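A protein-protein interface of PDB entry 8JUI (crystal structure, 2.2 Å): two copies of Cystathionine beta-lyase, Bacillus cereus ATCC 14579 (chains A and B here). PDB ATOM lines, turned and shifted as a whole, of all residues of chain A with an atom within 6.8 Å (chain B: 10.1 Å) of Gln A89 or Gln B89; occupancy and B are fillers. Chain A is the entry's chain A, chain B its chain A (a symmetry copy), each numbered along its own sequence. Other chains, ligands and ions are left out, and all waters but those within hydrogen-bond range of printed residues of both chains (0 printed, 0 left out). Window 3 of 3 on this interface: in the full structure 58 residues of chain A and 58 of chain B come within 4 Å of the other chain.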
ATOM      1  N   LEU A  87     -27.697  -2.962  -6.049  1.00  0.00           N
ATOM      2  CA  LEU A  87     -27.103  -2.070  -5.015  1.00  0.00           C
ATOM      3  C   LEU A  87     -25.768  -1.535  -5.535  1.00  0.00           C
ATOM      4  O   LEU A  87     -25.175  -2.180  -6.454  1.00  0.00           O
ATOM      5  CB  LEU A  87     -26.867  -2.866  -3.729  1.00  0.00           C
ATOM      6  CG  LEU A  87     -28.080  -3.602  -3.155  1.00  0.00           C
ATOM      7  CD1 LEU A  87     -27.720  -4.285  -1.845  1.00  0.00           C
ATOM      8  CD2 LEU A  87     -29.255  -2.661  -2.954  1.00  0.00           C
ATOM      9  N   SER A  88     -25.302  -0.429  -4.951  1.00  0.00           N
ATOM     10  CA  SER A  88     -23.979   0.195  -5.218  1.00  0.00           C
ATOM     11  C   SER A  88     -23.196   0.361  -3.913  1.00  0.00           C
ATOM     12  O   SER A  88     -23.765   0.095  -2.829  1.00  0.00           O
ATOM     13  CB  SER A  88     -24.163   1.469  -5.939  1.00  0.00           C
ATOM     14  OG  SER A  88     -25.108   1.302  -6.982  1.00  0.00           O
ATOM     15  N   GLN A  89     -21.910   0.713  -3.990  1.00  0.00           N
ATOM     16  CA  GLN A  89     -21.080   0.866  -2.769  1.00  0.00           C
ATOM     17  C   GLN A  89     -21.711   1.989  -1.933  1.00  0.00           C
ATOM     18  O   GLN A  89     -22.316   2.925  -2.513  1.00  0.00           O
ATOM     19  CB  GLN A  89     -19.612   1.159  -3.077  1.00  0.00           C
ATOM     20  CG  GLN A  89     -19.315   2.638  -3.192  1.00  0.00           C
ATOM     21  CD  GLN A  89     -17.943   2.916  -3.739  1.00  0.00           C
ATOM     22  OE1 GLN A  89     -17.835   3.542  -4.793  1.00  0.00           O
ATOM     23  NE2 GLN A  89     -16.910   2.432  -3.048  1.00  0.00           N
ATOM     24  N   GLY A  90     -21.664   1.833  -0.619  1.00  0.00           N
ATOM     25  CA  GLY A  90     -22.385   2.716   0.313  1.00  0.00           C
ATOM     26  C   GLY A  90     -23.691   2.115   0.805  1.00  0.00           C
ATOM     27  O   GLY A  90     -24.043   2.410   1.958  1.00  0.00           O
ATOM     28  N   ASP A  91     -24.408   1.362  -0.043  1.00  0.00           N
ATOM     29  CA  ASP A  91     -25.733   0.758   0.275  1.00  0.00           C
ATOM     30  C   ASP A  91     -25.599  -0.246   1.422  1.00  0.00           C
ATOM     31  O   ASP A  91     -24.591  -0.925   1.513  1.00  0.00           O
ATOM     32  CB  ASP A  91     -26.361   0.097  -0.949  1.00  0.00           C
ATOM     33  CG  ASP A  91     -26.831   1.109  -1.958  1.00  0.00           C
ATOM     34  OD1 ASP A  91     -26.797   2.309  -1.620  1.00  0.00           O
ATOM     35  OD2 ASP A  91     -27.224   0.699  -3.064  1.00  0.00           O
ATOM     36  N   LEU A 111     -19.711  -8.925  -1.544  1.00  0.00           N
ATOM     37  CA  LEU A 111     -20.283  -7.560  -1.645  1.00  0.00           C
ATOM     38  C   LEU A 111     -19.685  -6.680  -0.528  1.00  0.00           C
ATOM     39  O   LEU A 111     -19.743  -5.467  -0.660  1.00  0.00           O
ATOM     40  CB  LEU A 111     -21.809  -7.651  -1.578  1.00  0.00           C
ATOM     41  CG  LEU A 111     -22.467  -8.397  -2.744  1.00  0.00           C
ATOM     42  CD1 LEU A 111     -23.842  -8.909  -2.362  1.00  0.00           C
ATOM     43  CD2 LEU A 111     -22.566  -7.504  -3.956  1.00  0.00           C
ATOM     44  N   SER A 112     -19.122  -7.277   0.524  1.00  0.00           N
ATOM     45  CA  SER A 112     -18.399  -6.542   1.589  1.00  0.00           C
ATOM     46  C   SER A 112     -17.124  -5.873   1.026  1.00  0.00           C
ATOM     47  O   SER A 112     -16.742  -4.813   1.550  1.00  0.00           O
ATOM     48  CB  SER A 112     -18.118  -7.450   2.724  1.00  0.00           C
ATOM     49  OG  SER A 112     -17.333  -8.536   2.291  1.00  0.00           O
ATOM     50  N   ARG A 113     -16.522  -6.414  -0.049  1.00  0.00           N
ATOM     51  CA  ARG A 113     -15.298  -5.849  -0.686  1.00  0.00           C
ATOM     52  C   ARG A 113     -15.666  -4.689  -1.618  1.00  0.00           C
ATOM     53  O   ARG A 113     -14.754  -4.066  -2.166  1.00  0.00           O
ATOM     54  CB  ARG A 113     -14.499  -6.931  -1.413  1.00  0.00           C
ATOM     55  CG  ARG A 113     -14.043  -8.047  -0.495  1.00  0.00           C
ATOM     56  CD  ARG A 113     -13.177  -9.063  -1.177  1.00  0.00           C
ATOM     57  NE  ARG A 113     -13.890  -9.873  -2.156  1.00  0.00           N
ATOM     58  CZ  ARG A 113     -13.887  -9.710  -3.482  1.00  0.00           C
ATOM     59  NH1 ARG A 113     -13.189  -8.755  -4.077  1.00  0.00           N
ATOM     60  NH2 ARG A 113     -14.588 -10.545  -4.225  1.00  0.00           N
ATOM     61  N   TYR A 114     -16.950  -4.408  -1.806  1.00  0.00           N
ATOM     62  CA  TYR A 114     -17.452  -3.403  -2.773  1.00  0.00           C
ATOM     63  C   TYR A 114     -18.230  -2.304  -2.044  1.00  0.00           C
ATOM     64  O   TYR A 114     -18.951  -1.532  -2.707  1.00  0.00           O
ATOM     65  CB  TYR A 114     -18.292  -4.105  -3.845  1.00  0.00           C
ATOM     66  CG  TYR A 114     -17.493  -5.074  -4.685  1.00  0.00           C
ATOM     67  CD1 TYR A 114     -16.388  -4.652  -5.415  1.00  0.00           C
ATOM     68  CD2 TYR A 114     -17.801  -6.427  -4.704  1.00  0.00           C
ATOM     69  CE1 TYR A 114     -15.625  -5.548  -6.147  1.00  0.00           C
ATOM     70  CE2 TYR A 114     -17.048  -7.337  -5.428  1.00  0.00           C
ATOM     71  CZ  TYR A 114     -15.970  -6.893  -6.172  1.00  0.00           C
ATOM     72  OH  TYR A 114     -15.243  -7.790  -6.900  1.00  0.00           O
ATOM     73  N   GLY A 115     -18.074  -2.236  -0.723  1.00  0.00           N
ATOM     74  CA  GLY A 115     -18.704  -1.217   0.138  1.00  0.00           C
ATOM     75  C   GLY A 115     -20.206  -1.416   0.283  1.00  0.00           C
ATOM     76  O   GLY A 115     -20.899  -0.404   0.523  1.00  0.00           O
ATOM     77  N   VAL A 116     -20.714  -2.637   0.077  1.00  0.00           N
ATOM     78  CA  VAL A 116     -22.126  -2.981   0.416  1.00  0.00           C
ATOM     79  C   VAL A 116     -22.073  -3.613   1.804  1.00  0.00           C
ATOM     80  O   VAL A 116     -21.440  -4.689   1.959  1.00  0.00           O
ATOM     81  CB  VAL A 116     -22.805  -3.886  -0.636  1.00  0.00           C
ATOM     82  CG1 VAL A 116     -24.237  -4.237  -0.236  1.00  0.00           C
ATOM     83  CG2 VAL A 116     -22.797  -3.251  -2.028  1.00  0.00           C
ATOM     84  N   PHE B  84     -13.121 -10.467 -12.757  1.00  0.00           N
ATOM     85  CA  PHE B  84     -13.065  -9.080 -12.224  1.00  0.00           C
ATOM     86  C   PHE B  84     -13.440  -9.034 -10.735  1.00  0.00           C
ATOM     87  O   PHE B  84     -13.072  -8.063 -10.074  1.00  0.00           O
ATOM     88  CB  PHE B  84     -14.017  -8.160 -12.963  1.00  0.00           C
ATOM     89  CG  PHE B  84     -13.557  -7.704 -14.318  1.00  0.00           C
ATOM     90  CD1 PHE B  84     -12.264  -7.261 -14.525  1.00  0.00           C
ATOM     91  CD2 PHE B  84     -14.457  -7.626 -15.368  1.00  0.00           C
ATOM     92  CE1 PHE B  84     -11.856  -6.816 -15.770  1.00  0.00           C
ATOM     93  CE2 PHE B  84     -14.053  -7.169 -16.612  1.00  0.00           C
ATOM     94  CZ  PHE B  84     -12.754  -6.762 -16.807  1.00  0.00           C
ATOM     95  N   LEU B  85     -14.161 -10.025 -10.201  1.00  0.00           N
ATOM     96  CA  LEU B  85     -14.537 -10.007  -8.762  1.00  0.00           C
ATOM     97  C   LEU B  85     -13.302 -10.317  -7.920  1.00  0.00           C
ATOM     98  O   LEU B  85     -13.405 -10.309  -6.684  1.00  0.00           O
ATOM     99  CB  LEU B  85     -15.671 -10.989  -8.467  1.00  0.00           C
ATOM    100  CG  LEU B  85     -16.997 -10.678  -9.157  1.00  0.00           C
ATOM    101  CD1 LEU B  85     -18.073 -11.623  -8.660  1.00  0.00           C
ATOM    102  CD2 LEU B  85     -17.435  -9.230  -8.961  1.00  0.00           C
ATOM    103  N   LEU B  86     -12.174 -10.576  -8.563  1.00  0.00           N
ATOM    104  CA  LEU B  86     -10.868 -10.730  -7.881  1.00  0.00           C
ATOM    105  C   LEU B  86     -10.416  -9.358  -7.328  1.00  0.00           C
ATOM    106  O   LEU B  86      -9.600  -9.356  -6.403  1.00  0.00           O
ATOM    107  CB  LEU B  86      -9.846 -11.293  -8.871  1.00  0.00           C
ATOM    108  CG  LEU B  86      -9.893 -12.800  -9.140  1.00  0.00           C
ATOM    109  CD1 LEU B  86      -8.850 -13.201 -10.170  1.00  0.00           C
ATOM    110  CD2 LEU B  86      -9.666 -13.607  -7.885  1.00  0.00           C
ATOM    111  N   LEU B  87     -10.912  -8.259  -7.887  1.00  0.00           N
ATOM    112  CA  LEU B  87     -10.624  -6.860  -7.467  1.00  0.00           C
ATOM    113  C   LEU B  87     -11.602  -6.467  -6.359  1.00  0.00           C
ATOM    114  O   LEU B  87     -12.691  -7.112  -6.257  1.00  0.00           O
ATOM    115  CB  LEU B  87     -10.806  -5.922  -8.664  1.00  0.00           C
ATOM    116  CG  LEU B  87     -10.009  -6.269  -9.924  1.00  0.00           C
ATOM    117  CD1 LEU B  87     -10.227  -5.217 -11.000  1.00  0.00           C
ATOM    118  CD2 LEU B  87      -8.528  -6.415  -9.621  1.00  0.00           C
ATOM    119  N   SER B  88     -11.246  -5.437  -5.590  1.00  0.00           N
ATOM    120  CA  SER B  88     -12.090  -4.817  -4.534  1.00  0.00           C
ATOM    121  C   SER B  88     -12.229  -3.312  -4.779  1.00  0.00           C
ATOM    122  O   SER B  88     -11.560  -2.786  -5.698  1.00  0.00           O
ATOM    123  CB  SER B  88     -11.535  -5.128  -3.202  1.00  0.00           C
ATOM    124  OG  SER B  88     -11.182  -6.499  -3.134  1.00  0.00           O
ATOM    125  N   GLN B  89     -13.118  -2.634  -4.050  1.00  0.00           N
ATOM    126  CA  GLN B  89     -13.330  -1.179  -4.251  1.00  0.00           C
ATOM    127  C   GLN B  89     -11.998  -0.483  -3.934  1.00  0.00           C
ATOM    128  O   GLN B  89     -11.226  -0.986  -3.079  1.00  0.00           O
ATOM    129  CB  GLN B  89     -14.468  -0.617  -3.400  1.00  0.00           C
ATOM    130  CG  GLN B  89     -14.009  -0.134  -2.042  1.00  0.00           C
ATOM    131  CD  GLN B  89     -15.153   0.181  -1.119  1.00  0.00           C
ATOM    132  OE1 GLN B  89     -15.262  -0.446  -0.066  1.00  0.00           O
ATOM    133  NE2 GLN B  89     -16.012   1.119  -1.523  1.00  0.00           N
ATOM    134  N   GLY B  90     -11.699   0.570  -4.678  1.00  0.00           N
ATOM    135  CA  GLY B  90     -10.384   1.231  -4.632  1.00  0.00           C
ATOM    136  C   GLY B  90      -9.472   0.810  -5.772  1.00  0.00           C
ATOM    137  O   GLY B  90      -8.677   1.664  -6.197  1.00  0.00           O
ATOM    138  N   ASP B  91      -9.533  -0.458  -6.206  1.00  0.00           N
ATOM    139  CA  ASP B  91      -8.662  -1.032  -7.270  1.00  0.00           C
ATOM    140  C   ASP B  91      -8.907  -0.319  -8.601  1.00  0.00           C
ATOM    141  O   ASP B  91     -10.031   0.060  -8.883  1.00  0.00           O
ATOM    142  CB  ASP B  91      -8.867  -2.536  -7.419  1.00  0.00           C
ATOM    143  CG  ASP B  91      -8.302  -3.302  -6.254  1.00  0.00           C
ATOM    144  OD1 ASP B  91      -7.627  -2.661  -5.424  1.00  0.00           O
ATOM    145  OD2 ASP B  91      -8.537  -4.521  -6.181  1.00  0.00           O
ATOM    146  N   HIS B  92      -7.842  -0.117  -9.379  1.00  0.00           N
ATOM    147  CA  HIS B  92      -7.854   0.535 -10.718  1.00  0.00           C
ATOM    148  C   HIS B  92      -7.433  -0.469 -11.792  1.00  0.00           C
ATOM    149  O   HIS B  92      -6.495  -1.248 -11.536  1.00  0.00           O
ATOM    150  CB  HIS B  92      -6.899   1.733 -10.703  1.00  0.00           C
ATOM    151  CG  HIS B  92      -6.605   2.339 -12.032  1.00  0.00           C
ATOM    152  ND1 HIS B  92      -7.484   3.194 -12.651  1.00  0.00           N
ATOM    153  CD2 HIS B  92      -5.488   2.312 -12.805  1.00  0.00           C
ATOM    154  CE1 HIS B  92      -6.967   3.603 -13.803  1.00  0.00           C
ATOM    155  NE2 HIS B  92      -5.726   3.111 -13.891  1.00  0.00           N
ATOM    156  N   VAL B  93      -8.023  -0.348 -12.977  1.00  0.00           N
ATOM    157  CA  VAL B  93      -7.832  -1.298 -14.102  1.00  0.00           C
ATOM    158  C   VAL B  93      -7.335  -0.532 -15.327  1.00  0.00           C
ATOM    159  O   VAL B  93      -8.069   0.342 -15.783  1.00  0.00           O
ATOM    160  CB  VAL B  93      -9.145  -2.033 -14.435  1.00  0.00           C
ATOM    161  CG1 VAL B  93      -8.949  -3.013 -15.594  1.00  0.00           C
ATOM    162  CG2 VAL B  93      -9.712  -2.735 -13.205  1.00  0.00           C
ATOM    163  N   GLU B 109     -20.332   0.214 -16.386  1.00  0.00           N
ATOM    164  CA  GLU B 109     -21.714   0.314 -15.837  1.00  0.00           C
ATOM    165  C   GLU B 109     -21.882  -0.484 -14.536  1.00  0.00           C
ATOM    166  O   GLU B 109     -22.742  -0.119 -13.726  1.00  0.00           O
ATOM    167  CB  GLU B 109     -22.730  -0.040 -16.916  1.00  0.00           C
ATOM    168  CG  GLU B 109     -22.580   0.794 -18.171  1.00  0.00           C
ATOM    169  CD  GLU B 109     -23.758   0.690 -19.114  1.00  0.00           C
ATOM    170  OE1 GLU B 109     -23.544   0.348 -20.305  1.00  0.00           O
ATOM    171  OE2 GLU B 109     -24.896   0.948 -18.664  1.00  0.00           O
ATOM    172  N   VAL B 110     -21.046  -1.467 -14.245  1.00  0.00           N
ATOM    173  CA  VAL B 110     -21.268  -2.289 -13.031  1.00  0.00           C
ATOM    174  C   VAL B 110     -20.149  -2.033 -12.044  1.00  0.00           C
ATOM    175  O   VAL B 110     -20.454  -1.624 -10.912  1.00  0.00           O
ATOM    176  CB  VAL B 110     -21.390  -3.797 -13.314  1.00  0.00           C
ATOM    177  CG1 VAL B 110     -21.657  -4.546 -12.021  1.00  0.00           C
ATOM    178  CG2 VAL B 110     -22.441  -4.111 -14.377  1.00  0.00           C
ATOM    179  N   LEU B 111     -18.915  -2.338 -12.418  1.00  0.00           N
ATOM    180  CA  LEU B 111     -17.805  -2.309 -11.433  1.00  0.00           C
ATOM    181  C   LEU B 111     -17.500  -0.842 -11.062  1.00  0.00           C
ATOM    182  O   LEU B 111     -16.892  -0.627 -10.025  1.00  0.00           O
ATOM    183  CB  LEU B 111     -16.596  -3.038 -12.019  1.00  0.00           C
ATOM    184  CG  LEU B 111     -16.802  -4.535 -12.276  1.00  0.00           C
ATOM    185  CD1 LEU B 111     -15.823  -5.054 -13.312  1.00  0.00           C
ATOM    186  CD2 LEU B 111     -16.658  -5.317 -10.993  1.00  0.00           C
ATOM    187  N   SER B 112     -17.921   0.124 -11.880  1.00  0.00           N
ATOM    188  CA  SER B 112     -17.805   1.567 -11.564  1.00  0.00           C
ATOM    189  C   SER B 112     -18.681   1.935 -10.344  1.00  0.00           C
ATOM    190  O   SER B 112     -18.298   2.861  -9.609  1.00  0.00           O
ATOM    191  CB  SER B 112     -18.126   2.373 -12.765  1.00  0.00           C
ATOM    192  OG  SER B 112     -19.437   2.093 -13.197  1.00  0.00           O
ATOM    193  N   ARG B 113     -19.775   1.197 -10.080  1.00  0.00           N
ATOM    194  CA  ARG B 113     -20.685   1.448  -8.925  1.00  0.00           C
ATOM    195  C   ARG B 113     -20.104   0.840  -7.644  1.00  0.00           C
ATOM    196  O   ARG B 113     -20.706   1.025  -6.584  1.00  0.00           O
ATOM    197  CB  ARG B 113     -22.098   0.936  -9.208  1.00  0.00           C
ATOM    198  CG  ARG B 113     -22.732   1.590 -10.420  1.00  0.00           C
ATOM    199  CD  ARG B 113     -24.152   1.168 -10.649  1.00  0.00           C
ATOM    200  NE  ARG B 113     -24.286  -0.222 -11.066  1.00  0.00           N
ATOM    201  CZ  ARG B 113     -24.625  -1.258 -10.292  1.00  0.00           C
ATOM    202  NH1 ARG B 113     -24.902  -1.120  -9.005  1.00  0.00           N
ATOM    203  NH2 ARG B 113     -24.707  -2.456 -10.839  1.00  0.00           N
ATOM    204  N   TYR B 114     -18.986   0.129  -7.727  1.00  0.00           N
ATOM    205  CA  TYR B 114     -18.385  -0.618  -6.598  1.00  0.00           C
ATOM    206  C   TYR B 114     -16.981  -0.090  -6.295  1.00  0.00           C
ATOM    207  O   TYR B 114     -16.223  -0.766  -5.571  1.00  0.00           O
ATOM    208  CB  TYR B 114     -18.392  -2.116  -6.921  1.00  0.00           C
ATOM    209  CG  TYR B 114     -19.784  -2.688  -7.057  1.00  0.00           C
ATOM    210  CD1 TYR B 114     -20.698  -2.613  -6.013  1.00  0.00           C
ATOM    211  CD2 TYR B 114     -20.213  -3.249  -8.252  1.00  0.00           C
ATOM    212  CE1 TYR B 114     -21.991  -3.094  -6.153  1.00  0.00           C
ATOM    213  CE2 TYR B 114     -21.502  -3.731  -8.410  1.00  0.00           C
ATOM    214  CZ  TYR B 114     -22.388  -3.676  -7.349  1.00  0.00           C
ATOM    215  OH  TYR B 114     -23.651  -4.170  -7.503  1.00  0.00           O
ATOM    216  N   GLY B 115     -16.657   1.088  -6.826  1.00  0.00           N
ATOM    217  CA  GLY B 115     -15.370   1.775  -6.606  1.00  0.00           C
ATOM    218  C   GLY B 115     -14.208   1.090  -7.311  1.00  0.00           C
ATOM    219  O   GLY B 115     -13.070   1.235  -6.818  1.00  0.00           O
ATOM    220  N   VAL B 116     -14.469   0.314  -8.371  1.00  0.00           N
ATOM    221  CA  VAL B 116     -13.392  -0.210  -9.260  1.00  0.00           C
ATOM    222  C   VAL B 116     -13.312   0.768 -10.429  1.00  0.00           C
ATOM    223  O   VAL B 116     -14.308   0.898 -11.185  1.00  0.00           O
ATOM    224  CB  VAL B 116     -13.623  -1.670  -9.707  1.00  0.00           C
ATOM    225  CG1 VAL B 116     -12.513  -2.157 -10.638  1.00  0.00           C
ATOM    226  CG2 VAL B 116     -13.752  -2.621  -8.515  1.00  0.00           C
ATOM    227  N   SER B 117     -12.202   1.505 -10.524  1.00  0.00           N
ATOM    228  CA  SER B 117     -12.023   2.540 -11.578  1.00  0.00           C
ATOM    229  C   SER B 117     -11.188   1.941 -12.708  1.00  0.00           C
ATOM    230  O   SER B 117     -10.510   0.897 -12.498  1.00  0.00           O
ATOM    231  CB  SER B 117     -11.365   3.795 -11.050  1.00  0.00           C
ATOM    232  OG  SER B 117     -10.159   3.441 -10.410  1.00  0.00           O
ATOM    233  N   ASN B 136      -2.812   2.564  -7.323  1.00  0.00           N
ATOM    234  CA  ASN B 136      -3.843   1.527  -7.001  1.00  0.00           C
ATOM    235  C   ASN B 136      -4.149   0.647  -8.247  1.00  0.00           C
ATOM    236  O   ASN B 136      -5.152  -0.122  -8.197  1.00  0.00           O
ATOM    237  CB  ASN B 136      -5.086   2.221  -6.437  1.00  0.00           C
ATOM    238  CG  ASN B 136      -5.653   3.254  -7.383  1.00  0.00           C
ATOM    239  OD1 ASN B 136      -4.917   3.879  -8.144  1.00  0.00           O
ATOM    240  ND2 ASN B 136      -6.961   3.444  -7.356  1.00  0.00           N
ATOM    241  N   LYS B 138      -4.282  -2.446 -10.237  1.00  0.00           N
ATOM    242  CA  LYS B 138      -4.112  -3.868  -9.830  1.00  0.00           C
ATOM    243  C   LYS B 138      -4.219  -4.805 -11.037  1.00  0.00           C
ATOM    244  O   LYS B 138      -3.872  -6.009 -10.906  1.00  0.00           O
ATOM    245  CB  LYS B 138      -5.161  -4.265  -8.789  1.00  0.00           C
ATOM    246  CG  LYS B 138      -5.100  -3.510  -7.467  1.00  0.00           C
ATOM    247  CD  LYS B 138      -3.759  -3.587  -6.760  1.00  0.00           C
ATOM    248  CE  LYS B 138      -3.660  -2.607  -5.610  1.00  0.00           C
ATOM    249  NZ  LYS B 138      -2.914  -3.207  -4.480  1.00  0.00           N
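No residue of chain B comes within 4 Å of Asp A91.
Printed residues of chain B within 4 Å of Arg A113: Leu B85, Leu B87, Ser B88 and Gln B89.
Of the printed residues of chain A, Leu B87 touches Arg A113 (2.8 Å) and Tyr A114 (2.7 Å).
Gln B89 touches just these residues of chain A: Gln A89, Arg A113 and Gly A115.
Val B110 touches none of the printed residues of chain A.
Of the printed residues of chain A, Arg B113 touches Leu A87 (2.8 Å), Ser A88 (3.2 Å) and Gln A89 (2.9 Å).
Of the printed residues of chain A, Tyr B114 touches Leu A87, Ser A88 and Tyr A114.
Of the printed residues of chain A, Gly B115 touches Gln A89.
The nearest residue of chain B that does not touch Gln A89 is Tyr B114 (4.02 Å).
The backbone NH (N) of Ser B88 sits at hydrogen-bond distance from the side-chain carboxylate (OD2) of Asp B91 (2.9 Å).
The side-chain carboxylate of Asp A91 lies within hydrogen-bond range of the backbone NH of Ser A88, 2.9 Å away.
The backbone carbonyl oxygen (O) of Gly B115 sits at hydrogen-bond distance from the backbone NH (N) of Gly B90.
The backbone carbonyl oxygen (O) of Gly A115 lies within hydrogen-bond range of the backbone NH (N) of Gly A90, 2.6 Å away.
The guanidinium group (NE) of Arg B113 is in hydrogen-bond range of the backbone carbonyl oxygen (O) of Glu B109, at 3.1 Å.
Of the 11 printed residues of chain A, 6 touch a printed residue of chain B.
Of the 21 printed residues of chain B, 8 touch a printed residue of chain A.
Printed residues of chain B that touch a printed residue of chain A: Phe B84, Leu B85, Leu B87, Ser B88, Gln B89, Arg B113, Tyr B114 and Gly B115.
Hydrophobic or aromatic side chains of chain B within 4 Å of the printed part of chain A: Leu B85 and Tyr B114.
Among the printed residues, no Asp or Glu carboxylate lies within 4 Å of a Lys or Arg side-chain nitrogen of the other chain.
Among the printed residues, merely in contact across the chains: Ser A88 with Tyr B114 (3.96 Å), Tyr A114 with Phe B84 (3.9 Å), Tyr A114 with Ser B88 (3.95 Å) and Tyr A114 with Tyr B114 (3.6 Å).
Leu A87 touches Arg B113, and with the chains exchanged Arg A113 touches Leu B87.
Leu A87 touches Tyr B114, and with the chains exchanged Tyr A114 touches Leu B87.
Gln B89 touches its own counterpart, Gln A89.
Gln A89 touches Arg B113, and with the chains exchanged Arg A113 touches Gln B89.
NH1 of Arg B113 is in hydrogen-bond range of O of Leu A87, 2.8 Å away.
NH1 of Arg A113 sits at hydrogen-bond distance from O of Leu B87 (2.8 Å).
The guanidinium group (NH1) of Arg A113 sits at hydrogen-bond distance from the side-chain hydroxyl (OG) of Ser B88 (3.2 Å).
The side-chain hydroxyl of Tyr A114 is in hydrogen-bond range of the backbone carbonyl oxygen of Leu B87 (2.7 Å).
O of Leu B85 lies close to OH of Tyr A114 (3.1 Å).
The backbone carbonyl oxygen of Arg A113 sits at hydrogen-bond distance from the backbone NH of Gln B89.
The side-chain amide nitrogen of Gln A89 lies close to the side-chain amide nitrogen of Gln B89 (2.2 Å).
N of Gly A115 is in hydrogen-bond range of OE1 of Gln B89 (3.4 Å).
O of Leu B85 lies within hydrogen-bond range of NH2 of Arg A113, at 2.7 Å.
The side-chain hydroxyl (OG) of Ser A88 is in hydrogen-bond range of the guanidinium group (NH1) of Arg B113.
O of Arg B113 sits at hydrogen-bond distance from N of Gln A89 (2.9 Å).
OE1 of Gln A89 lies within hydrogen-bond range of N of Gly B115.
The backbone carbonyl oxygen (O) of Leu A87 sits at hydrogen-bond distance from the side-chain hydroxyl (OH) of Tyr B114, at 2.7 Å.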
